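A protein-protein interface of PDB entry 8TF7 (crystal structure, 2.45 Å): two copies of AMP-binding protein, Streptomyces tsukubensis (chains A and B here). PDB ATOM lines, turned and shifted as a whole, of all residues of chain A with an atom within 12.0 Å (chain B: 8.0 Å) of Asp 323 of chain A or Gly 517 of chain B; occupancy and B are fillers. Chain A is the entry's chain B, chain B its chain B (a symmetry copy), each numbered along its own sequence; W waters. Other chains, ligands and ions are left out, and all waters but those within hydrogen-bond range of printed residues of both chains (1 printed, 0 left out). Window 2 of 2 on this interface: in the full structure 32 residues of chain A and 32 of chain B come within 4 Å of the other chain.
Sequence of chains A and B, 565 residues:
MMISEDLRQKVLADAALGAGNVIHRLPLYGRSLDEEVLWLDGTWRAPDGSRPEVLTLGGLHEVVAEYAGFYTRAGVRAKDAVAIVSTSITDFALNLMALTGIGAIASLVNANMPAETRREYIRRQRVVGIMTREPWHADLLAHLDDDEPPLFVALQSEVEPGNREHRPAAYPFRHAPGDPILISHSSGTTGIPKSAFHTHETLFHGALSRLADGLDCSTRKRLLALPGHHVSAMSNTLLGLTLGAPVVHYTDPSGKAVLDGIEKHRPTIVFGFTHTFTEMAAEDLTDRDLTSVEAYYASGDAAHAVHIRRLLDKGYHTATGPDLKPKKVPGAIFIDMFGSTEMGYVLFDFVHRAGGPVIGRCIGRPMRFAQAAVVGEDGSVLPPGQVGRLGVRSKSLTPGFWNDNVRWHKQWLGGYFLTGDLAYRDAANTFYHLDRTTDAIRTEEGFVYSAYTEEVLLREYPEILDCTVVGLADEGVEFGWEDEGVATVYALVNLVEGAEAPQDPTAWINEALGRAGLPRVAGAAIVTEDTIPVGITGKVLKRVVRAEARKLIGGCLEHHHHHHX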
ATOM      1  N   THR A 318      34.026 -17.021   4.615  1.00  0.00           N
ATOM      2  CA  THR A 318      32.945 -17.704   5.308  1.00  0.00           C
ATOM      3  C   THR A 318      33.331 -17.945   6.762  1.00  0.00           C
ATOM      4  O   THR A 318      34.485 -18.261   7.065  1.00  0.00           O
ATOM      5  CB  THR A 318      32.613 -19.035   4.632  1.00  0.00           C
ATOM      6  OG1 THR A 318      32.198 -18.795   3.281  1.00  0.00           O
ATOM      7  CG2 THR A 318      31.504 -19.758   5.383  1.00  0.00           C
ATOM      8  N   ALA A 319      32.356 -17.797   7.654  1.00  0.00           N
ATOM      9  CA  ALA A 319      32.591 -17.944   9.080  1.00  0.00           C
ATOM     10  C   ALA A 319      31.338 -18.509   9.732  1.00  0.00           C
ATOM     11  O   ALA A 319      30.262 -18.553   9.132  1.00  0.00           O
ATOM     12  CB  ALA A 319      32.980 -16.608   9.722  1.00  0.00           C
ATOM     13  N   THR A 320      31.491 -18.940  10.978  1.00  0.00           N
ATOM     14  CA  THR A 320      30.399 -19.527  11.742  1.00  0.00           C
ATOM     15  C   THR A 320      29.715 -18.426  12.544  1.00  0.00           C
ATOM     16  O   THR A 320      30.364 -17.742  13.344  1.00  0.00           O
ATOM     17  CB  THR A 320      30.927 -20.631  12.658  1.00  0.00           C
ATOM     18  OG1 THR A 320      31.498 -21.677  11.859  1.00  0.00           O
ATOM     19  CG2 THR A 320      29.809 -21.202  13.519  1.00  0.00           C
ATOM     20  N   GLY A 321      28.414 -18.248  12.323  1.00  0.00           N
ATOM     21  CA  GLY A 321      27.667 -17.203  12.986  1.00  0.00           C
ATOM     22  C   GLY A 321      27.203 -17.617  14.364  1.00  0.00           C
ATOM     23  O   GLY A 321      27.329 -18.776  14.788  1.00  0.00           O
ATOM     24  N   PRO A 322      26.634 -16.653  15.094  1.00  0.00           N
ATOM     25  CA  PRO A 322      26.192 -16.941  16.471  1.00  0.00           C
ATOM     26  C   PRO A 322      25.175 -18.066  16.557  1.00  0.00           C
ATOM     27  O   PRO A 322      24.988 -18.628  17.643  1.00  0.00           O
ATOM     28  CB  PRO A 322      25.592 -15.609  16.945  1.00  0.00           C
ATOM     29  CG  PRO A 322      26.121 -14.573  16.004  1.00  0.00           C
ATOM     30  CD  PRO A 322      26.349 -15.264  14.693  1.00  0.00           C
ATOM     31  N   ASP A 323      24.511 -18.410  15.456  1.00  0.00           N
ATOM     32  CA  ASP A 323      23.611 -19.553  15.414  1.00  0.00           C
ATOM     33  C   ASP A 323      24.328 -20.844  15.029  1.00  0.00           C
ATOM     34  O   ASP A 323      23.665 -21.836  14.711  1.00  0.00           O
ATOM     35  CB  ASP A 323      22.466 -19.280  14.435  1.00  0.00           C
ATOM     36  CG  ASP A 323      22.955 -18.940  13.040  1.00  0.00           C
ATOM     37  OD1 ASP A 323      24.164 -18.674  12.877  1.00  0.00           O
ATOM     38  OD2 ASP A 323      22.128 -18.937  12.105  1.00  0.00           O
ATOM     39  N   LEU A 324      25.663 -20.852  15.059  1.00  0.00           N
ATOM     40  CA  LEU A 324      26.459 -22.024  14.694  1.00  0.00           C
ATOM     41  C   LEU A 324      26.151 -22.474  13.266  1.00  0.00           C
ATOM     42  O   LEU A 324      26.082 -23.669  12.971  1.00  0.00           O
ATOM     43  CB  LEU A 324      26.245 -23.174  15.684  1.00  0.00           C
ATOM     44  CG  LEU A 324      26.022 -22.802  17.150  1.00  0.00           C
ATOM     45  CD1 LEU A 324      25.492 -24.000  17.927  1.00  0.00           C
ATOM     46  CD2 LEU A 324      27.296 -22.278  17.791  1.00  0.00           C
ATOM     47  N   LYS A 325      25.972 -21.506  12.373  1.00  0.00           N
ATOM     48  CA  LYS A 325      25.679 -21.753  10.970  1.00  0.00           C
ATOM     49  C   LYS A 325      26.565 -20.876  10.097  1.00  0.00           C
ATOM     50  O   LYS A 325      27.017 -19.813  10.535  1.00  0.00           O
ATOM     51  CB  LYS A 325      24.200 -21.472  10.661  1.00  0.00           C
ATOM     52  CG  LYS A 325      23.278 -22.668  10.913  1.00  0.00           C
ATOM     53  CD  LYS A 325      21.954 -22.265  11.566  1.00  0.00           C
ATOM     54  CE  LYS A 325      20.763 -22.560  10.656  1.00  0.00           C
ATOM     55  NZ  LYS A 325      19.468 -22.575  11.401  1.00  0.00           N
ATOM     56  N   PRO A 326      26.841 -21.303   8.863  1.00  0.00           N
ATOM     57  CA  PRO A 326      27.724 -20.508   7.997  1.00  0.00           C
ATOM     58  C   PRO A 326      27.191 -19.100   7.777  1.00  0.00           C
ATOM     59  O   PRO A 326      25.983 -18.869   7.706  1.00  0.00           O
ATOM     60  CB  PRO A 326      27.752 -21.305   6.685  1.00  0.00           C
ATOM     61  CG  PRO A 326      27.403 -22.697   7.074  1.00  0.00           C
ATOM     62  CD  PRO A 326      26.454 -22.582   8.238  1.00  0.00           C
ATOM     63  N   LYS A 327      28.120 -18.154   7.663  1.00  0.00           N
ATOM     64  CA  LYS A 327      27.782 -16.748   7.486  1.00  0.00           C
ATOM     65  C   LYS A 327      28.835 -16.100   6.599  1.00  0.00           C
ATOM     66  O   LYS A 327      30.033 -16.221   6.868  1.00  0.00           O
ATOM     67  CB  LYS A 327      27.703 -16.034   8.840  1.00  0.00           C
ATOM     68  CG  LYS A 327      27.954 -14.538   8.783  1.00  0.00           C
ATOM     69  CD  LYS A 327      27.589 -13.871  10.104  1.00  0.00           C
ATOM     70  CE  LYS A 327      27.703 -12.357  10.011  1.00  0.00           C
ATOM     71  NZ  LYS A 327      26.387 -11.713   9.750  1.00  0.00           N
ATOM     72  N   LYS A 328      28.383 -15.422   5.545  1.00  0.00           N
ATOM     73  CA  LYS A 328      29.287 -14.719   4.643  1.00  0.00           C
ATOM     74  C   LYS A 328      29.724 -13.405   5.279  1.00  0.00           C
ATOM     75  O   LYS A 328      28.894 -12.651   5.796  1.00  0.00           O
ATOM     76  CB  LYS A 328      28.608 -14.461   3.300  1.00  0.00           C
ATOM     77  CG  LYS A 328      29.572 -14.105   2.174  1.00  0.00           C
ATOM     78  CD  LYS A 328      28.972 -13.081   1.216  1.00  0.00           C
ATOM     79  CE  LYS A 328      29.032 -13.559  -0.228  1.00  0.00           C
ATOM     80  NZ  LYS A 328      28.352 -12.606  -1.153  1.00  0.00           N
ATOM     81  N   VAL A 329      31.023 -13.128   5.232  1.00  0.00           N
ATOM     82  CA  VAL A 329      31.588 -11.971   5.923  1.00  0.00           C
ATOM     83  C   VAL A 329      32.487 -11.190   4.973  1.00  0.00           C
ATOM     84  O   VAL A 329      33.298 -11.793   4.256  1.00  0.00           O
ATOM     85  CB  VAL A 329      32.363 -12.413   7.178  1.00  0.00           C
ATOM     86  CG1 VAL A 329      33.110 -11.239   7.791  1.00  0.00           C
ATOM     87  CG2 VAL A 329      31.413 -13.047   8.188  1.00  0.00           C
ATOM     88  N   ILE B 359      31.904 -17.078  19.597  1.00  0.00           N
ATOM     89  CA  ILE B 359      30.888 -18.124  19.480  1.00  0.00           C
ATOM     90  C   ILE B 359      31.468 -19.396  20.092  1.00  0.00           C
ATOM     91  O   ILE B 359      32.297 -20.072  19.479  1.00  0.00           O
ATOM     92  CB  ILE B 359      30.458 -18.337  18.027  1.00  0.00           C
ATOM     93  CG1 ILE B 359      29.570 -17.179  17.569  1.00  0.00           C
ATOM     94  CG2 ILE B 359      29.730 -19.664  17.877  1.00  0.00           C
ATOM     95  CD1 ILE B 359      30.015 -16.541  16.279  1.00  0.00           C
ATOM     96  N   GLY B 385      33.347 -25.621  10.704  1.00  0.00           N
ATOM     97  CA  GLY B 385      32.027 -25.042  10.778  1.00  0.00           C
ATOM     98  C   GLY B 385      30.909 -26.005  11.114  1.00  0.00           C
ATOM     99  O   GLY B 385      29.764 -25.563  11.278  1.00  0.00           O
ATOM    100  N   VAL B 387      29.270 -29.000  13.699  1.00  0.00           N
ATOM    101  CA  VAL B 387      29.278 -29.462  15.080  1.00  0.00           C
ATOM    102  C   VAL B 387      29.440 -30.975  15.086  1.00  0.00           C
ATOM    103  O   VAL B 387      28.780 -31.686  14.317  1.00  0.00           O
ATOM    104  CB  VAL B 387      27.989 -29.045  15.808  1.00  0.00           C
ATOM    105  CG1 VAL B 387      28.031 -29.487  17.264  1.00  0.00           C
ATOM    106  CG2 VAL B 387      27.786 -27.542  15.702  1.00  0.00           C
ATOM    107  N   GLU B 445      13.149 -27.432  15.828  1.00  0.00           N
ATOM    108  CA  GLU B 445      13.951 -26.424  15.145  1.00  0.00           C
ATOM    109  C   GLU B 445      15.337 -26.964  14.821  1.00  0.00           C
ATOM    110  O   GLU B 445      15.794 -26.903  13.673  1.00  0.00           O
ATOM    111  CB  GLU B 445      14.067 -25.170  16.017  1.00  0.00           C
ATOM    112  CG  GLU B 445      12.768 -24.719  16.668  1.00  0.00           C
ATOM    113  CD  GLU B 445      12.992 -23.704  17.777  1.00  0.00           C
ATOM    114  OE1 GLU B 445      13.220 -24.123  18.932  1.00  0.00           O
ATOM    115  OE2 GLU B 445      12.940 -22.487  17.492  1.00  0.00           O
ATOM    116  N   PHE B 447      19.205 -28.632  17.083  1.00  0.00           N
ATOM    117  CA  PHE B 447      19.843 -28.991  18.341  1.00  0.00           C
ATOM    118  C   PHE B 447      20.094 -27.751  19.190  1.00  0.00           C
ATOM    119  O   PHE B 447      20.507 -26.703  18.686  1.00  0.00           O
ATOM    120  CB  PHE B 447      21.150 -29.737  18.087  1.00  0.00           C
ATOM    121  CG  PHE B 447      21.019 -31.226  18.200  1.00  0.00           C
ATOM    122  CD1 PHE B 447      20.969 -31.837  19.441  1.00  0.00           C
ATOM    123  CD2 PHE B 447      20.930 -32.016  17.065  1.00  0.00           C
ATOM    124  CE1 PHE B 447      20.842 -33.209  19.550  1.00  0.00           C
ATOM    125  CE2 PHE B 447      20.803 -33.387  17.165  1.00  0.00           C
ATOM    126  CZ  PHE B 447      20.757 -33.984  18.409  1.00  0.00           C
ATOM    127  N   TYR B 449      22.317 -26.501  22.375  1.00  0.00           N
ATOM    128  CA  TYR B 449      23.506 -26.814  23.160  1.00  0.00           C
ATOM    129  C   TYR B 449      23.432 -26.056  24.478  1.00  0.00           C
ATOM    130  O   TYR B 449      23.416 -24.820  24.492  1.00  0.00           O
ATOM    131  CB  TYR B 449      24.765 -26.470  22.368  1.00  0.00           C
ATOM    132  CG  TYR B 449      24.780 -27.155  21.017  1.00  0.00           C
ATOM    133  CD1 TYR B 449      25.069 -28.509  20.907  1.00  0.00           C
ATOM    134  CD2 TYR B 449      24.473 -26.455  19.856  1.00  0.00           C
ATOM    135  CE1 TYR B 449      25.069 -29.143  19.680  1.00  0.00           C
ATOM    136  CE2 TYR B 449      24.472 -27.081  18.624  1.00  0.00           C
ATOM    137  CZ  TYR B 449      24.771 -28.425  18.543  1.00  0.00           C
ATOM    138  OH  TYR B 449      24.772 -29.056  17.323  1.00  0.00           O
ATOM    139  N   TYR B 452      26.450 -23.624  25.625  1.00  0.00           N
ATOM    140  CA  TYR B 452      26.496 -22.474  24.731  1.00  0.00           C
ATOM    141  C   TYR B 452      25.251 -21.611  24.887  1.00  0.00           C
ATOM    142  O   TYR B 452      25.341 -20.380  24.971  1.00  0.00           O
ATOM    143  CB  TYR B 452      26.643 -22.925  23.281  1.00  0.00           C
ATOM    144  CG  TYR B 452      26.579 -21.767  22.316  1.00  0.00           C
ATOM    145  CD1 TYR B 452      27.535 -20.760  22.353  1.00  0.00           C
ATOM    146  CD2 TYR B 452      25.556 -21.666  21.385  1.00  0.00           C
ATOM    147  CE1 TYR B 452      27.482 -19.692  21.483  1.00  0.00           C
ATOM    148  CE2 TYR B 452      25.493 -20.600  20.508  1.00  0.00           C
ATOM    149  CZ  TYR B 452      26.459 -19.616  20.563  1.00  0.00           C
ATOM    150  OH  TYR B 452      26.401 -18.552  19.693  1.00  0.00           O
ATOM    151  N   VAL B 456      25.252 -17.735  26.068  1.00  0.00           N
ATOM    152  CA  VAL B 456      24.654 -16.644  25.301  1.00  0.00           C
ATOM    153  C   VAL B 456      23.761 -15.797  26.199  1.00  0.00           C
ATOM    154  O   VAL B 456      23.956 -14.584  26.336  1.00  0.00           O
ATOM    155  CB  VAL B 456      23.877 -17.203  24.094  1.00  0.00           C
ATOM    156  CG1 VAL B 456      22.727 -16.280  23.689  1.00  0.00           C
ATOM    157  CG2 VAL B 456      24.817 -17.420  22.919  1.00  0.00           C
ATOM    158  N   ASN B 510      13.643 -15.649  25.116  1.00  0.00           N
ATOM    159  CA  ASN B 510      13.539 -15.780  23.668  1.00  0.00           C
ATOM    160  C   ASN B 510      13.940 -14.510  22.932  1.00  0.00           C
ATOM    161  O   ASN B 510      14.217 -14.567  21.728  1.00  0.00           O
ATOM    162  CB  ASN B 510      12.112 -16.174  23.288  1.00  0.00           C
ATOM    163  CG  ASN B 510      11.766 -17.585  23.718  1.00  0.00           C
ATOM    164  OD1 ASN B 510      12.653 -18.390  24.002  1.00  0.00           O
ATOM    165  ND2 ASN B 510      10.477 -17.893  23.765  1.00  0.00           N
ATOM    166  N   GLU B 511      13.977 -13.365  23.618  1.00  0.00           N
ATOM    167  CA  GLU B 511      14.414 -12.137  22.962  1.00  0.00           C
ATOM    168  C   GLU B 511      15.907 -12.181  22.660  1.00  0.00           C
ATOM    169  O   GLU B 511      16.342 -11.742  21.590  1.00  0.00           O
ATOM    170  CB  GLU B 511      14.076 -10.928  23.835  1.00  0.00           C
ATOM    171  CG  GLU B 511      12.699 -10.336  23.564  1.00  0.00           C
ATOM    172  CD  GLU B 511      12.058  -9.747  24.807  1.00  0.00           C
ATOM    173  OE1 GLU B 511      12.796  -9.383  25.746  1.00  0.00           O
ATOM    174  OE2 GLU B 511      10.814  -9.647  24.842  1.00  0.00           O
ATOM    175  N   ALA B 512      16.705 -12.712  23.589  1.00  0.00           N
ATOM    176  CA  ALA B 512      18.136 -12.861  23.347  1.00  0.00           C
ATOM    177  C   ALA B 512      18.423 -14.027  22.408  1.00  0.00           C
ATOM    178  O   ALA B 512      19.265 -13.913  21.511  1.00  0.00           O
ATOM    179  CB  ALA B 512      18.874 -13.054  24.671  1.00  0.00           C
ATOM    180  N   LEU B 513      17.736 -15.156  22.602  1.00  0.00           N
ATOM    181  CA  LEU B 513      17.905 -16.282  21.693  1.00  0.00           C
ATOM    182  C   LEU B 513      17.551 -15.895  20.263  1.00  0.00           C
ATOM    183  O   LEU B 513      18.132 -16.430  19.313  1.00  0.00           O
ATOM    184  CB  LEU B 513      17.046 -17.459  22.148  1.00  0.00           C
ATOM    185  CG  LEU B 513      17.373 -18.028  23.530  1.00  0.00           C
ATOM    186  CD1 LEU B 513      16.281 -18.981  23.987  1.00  0.00           C
ATOM    187  CD2 LEU B 513      18.723 -18.725  23.519  1.00  0.00           C
ATOM    188  N   GLY B 514      16.605 -14.970  20.094  1.00  0.00           N
ATOM    189  CA  GLY B 514      16.241 -14.539  18.756  1.00  0.00           C
ATOM    190  C   GLY B 514      17.295 -13.653  18.121  1.00  0.00           C
ATOM    191  O   GLY B 514      17.569 -13.762  16.922  1.00  0.00           O
ATOM    192  N   ARG B 515      17.900 -12.761  18.911  1.00  0.00           N
ATOM    193  CA  ARG B 515      18.954 -11.905  18.380  1.00  0.00           C
ATOM    194  C   ARG B 515      20.100 -12.734  17.814  1.00  0.00           C
ATOM    195  O   ARG B 515      20.656 -12.405  16.760  1.00  0.00           O
ATOM    196  CB  ARG B 515      19.475 -10.967  19.468  1.00  0.00           C
ATOM    197  CG  ARG B 515      18.469  -9.941  19.955  1.00  0.00           C
ATOM    198  CD  ARG B 515      18.881  -9.384  21.310  1.00  0.00           C
ATOM    199  NE  ARG B 515      17.733  -8.948  22.094  1.00  0.00           N
ATOM    200  CZ  ARG B 515      17.667  -8.989  23.419  1.00  0.00           C
ATOM    201  NH1 ARG B 515      18.671  -9.447  24.149  1.00  0.00           N
ATOM    202  NH2 ARG B 515      16.566  -8.555  24.027  1.00  0.00           N
ATOM    203  N   ALA B 516      20.471 -13.809  18.508  1.00  0.00           N
ATOM    204  CA  ALA B 516      21.551 -14.680  18.066  1.00  0.00           C
ATOM    205  C   ALA B 516      21.096 -15.722  17.055  1.00  0.00           C
ATOM    206  O   ALA B 516      21.926 -16.510  16.589  1.00  0.00           O
ATOM    207  CB  ALA B 516      22.184 -15.378  19.272  1.00  0.00           C
ATOM    208  N   GLY B 517      19.814 -15.746  16.702  1.00  0.00           N
ATOM    209  CA  GLY B 517      19.320 -16.746  15.779  1.00  0.00           C
ATOM    210  C   GLY B 517      19.232 -18.138  16.356  1.00  0.00           C
ATOM    211  O   GLY B 517      19.110 -19.106  15.602  1.00  0.00           O
ATOM    212  N   LEU B 518      19.288 -18.268  17.676  1.00  0.00           N
ATOM    213  CA  LEU B 518      19.271 -19.582  18.295  1.00  0.00           C
ATOM    214  C   LEU B 518      17.839 -20.089  18.449  1.00  0.00           C
ATOM    215  O   LEU B 518      16.894 -19.299  18.513  1.00  0.00           O
ATOM    216  CB  LEU B 518      19.944 -19.532  19.661  1.00  0.00           C
ATOM    217  CG  LEU B 518      21.471 -19.453  19.659  1.00  0.00           C
ATOM    218  CD1 LEU B 518      21.999 -19.215  21.066  1.00  0.00           C
ATOM    219  CD2 LEU B 518      22.068 -20.718  19.063  1.00  0.00           C
ATOM    220  N   PRO B 519      17.655 -21.408  18.493  1.00  0.00           N
ATOM    221  CA  PRO B 519      16.326 -21.950  18.800  1.00  0.00           C
ATOM    222  C   PRO B 519      15.799 -21.381  20.111  1.00  0.00           C
ATOM    223  O   PRO B 519      16.544 -21.204  21.077  1.00  0.00           O
ATOM    224  CB  PRO B 519      16.560 -23.462  18.895  1.00  0.00           C
ATOM    225  CG  PRO B 519      17.867 -23.725  18.236  1.00  0.00           C
ATOM    226  CD  PRO B 519      18.631 -22.445  18.111  1.00  0.00           C
ATOM    227  N   ARG B 520      14.504 -21.093  20.139  1.00  0.00           N
ATOM    228  CA  ARG B 520      13.873 -20.487  21.301  1.00  0.00           C
ATOM    229  C   ARG B 520      13.335 -21.559  22.245  1.00  0.00           C
ATOM    230  O   ARG B 520      13.038 -22.686  21.842  1.00  0.00           O
ATOM    231  CB  ARG B 520      12.742 -19.554  20.863  1.00  0.00           C
ATOM    232  CG  ARG B 520      11.519 -20.271  20.309  1.00  0.00           C
ATOM    233  CD  ARG B 520      10.444 -20.439  21.377  1.00  0.00           C
ATOM    234  NE  ARG B 520       9.140 -20.766  20.810  1.00  0.00           N
ATOM    235  CZ  ARG B 520       7.984 -20.586  21.435  1.00  0.00           C
ATOM    236  NH1 ARG B 520       7.928 -20.075  22.655  1.00  0.00           N
ATOM    237  NH2 ARG B 520       6.854 -20.928  20.822  1.00  0.00           N
HETATM  238  O   HOH W   1      29.374 -22.688  10.327  1.00  0.00           O
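Water W1 lies within hydrogen-bond range of the side-chain hydroxyl (OG1) of Thr 320 of chain A and the backbone carbonyl oxygen (O) of Gly 385 of chain B.
No position is printed for both chains.
Of the 12 pairs that touch across the chains among the printed residues, none has its exchanged pair printed and touching as well.
The side-chain carboxylate of Asp 323 of chain A lies close to the backbone NH of Lys 325 of chain A, at 3.4 Å.
O of Leu 513 of chain B sits at hydrogen-bond distance from N of Leu 518 of chain B, at 2.7 Å.
Of the 19 printed residues of chain B, 7 touch a printed residue of chain A.
Hydrophobic or aromatic side chains of chain A that line the printed part of chain B: Pro 322 and Leu 324.
Ile 359 of chain B touches Thr 320 of chain A (CD1 to O, 3.2 Å).
OG1 of Thr 320 of chain A touches CA of Gly 385 of chain B (3.6 Å).
Gly 321 of chain A touches Ile 359 of chain B.
CA of Pro 322 of chain A touches CG1 of Ile 359 of chain B, at 3.6 Å.
Pro 322 of chain A touches Ala 516 of chain B.
O of Pro 322 of chain A touches CD2 of Leu 518 of chain B, 3.9 Å away.
Gly 517 of chain B touches Asp 323 of chain A (O to CB, 3.6 Å).
Leu 324 of chain A touches Ile 359 of chain B.
Leu 324 of chain A touches Tyr 449 of chain B (CD1 to CD2, 3.3 Å).
Tyr 452 of chain B touches Leu 324 of chain A (CE2 to CD2, 3.7 Å).
OH of Tyr 452 of chain B lies within hydrogen-bond range of O of Pro 322 of chain A, at 2.5 Å.
O of Ala 516 of chain B lies within hydrogen-bond range of N of Asp 323 of chain A, 3.4 Å away.
Of chain B, only Ala 516 and Gly 517 come within 4 Å of Asp 323 of chain A.
Gly 517 of chain B touches just one residue of chain A: Asp 323.
Of chain A, only Pro 322 (3.9 Å) comes within 4 Å of Leu 518 of chain B.
Of the printed residues of chain B, Leu 324 of chain A touches Ile 359, Tyr 449 and Tyr 452.
Printed residues of chain B within 4 Å of Pro 322 of chain A: Ile 359, Tyr 452, Ala 516 and Leu 518.
Lys 325 of chain A touches none of the printed residues of chain B.
Val 387 of chain B touches none of the printed residues of chain A.
The nearest residue of chain A that does not touch Gly 517 of chain B is Lys 325 of chain A (5.5 Å).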
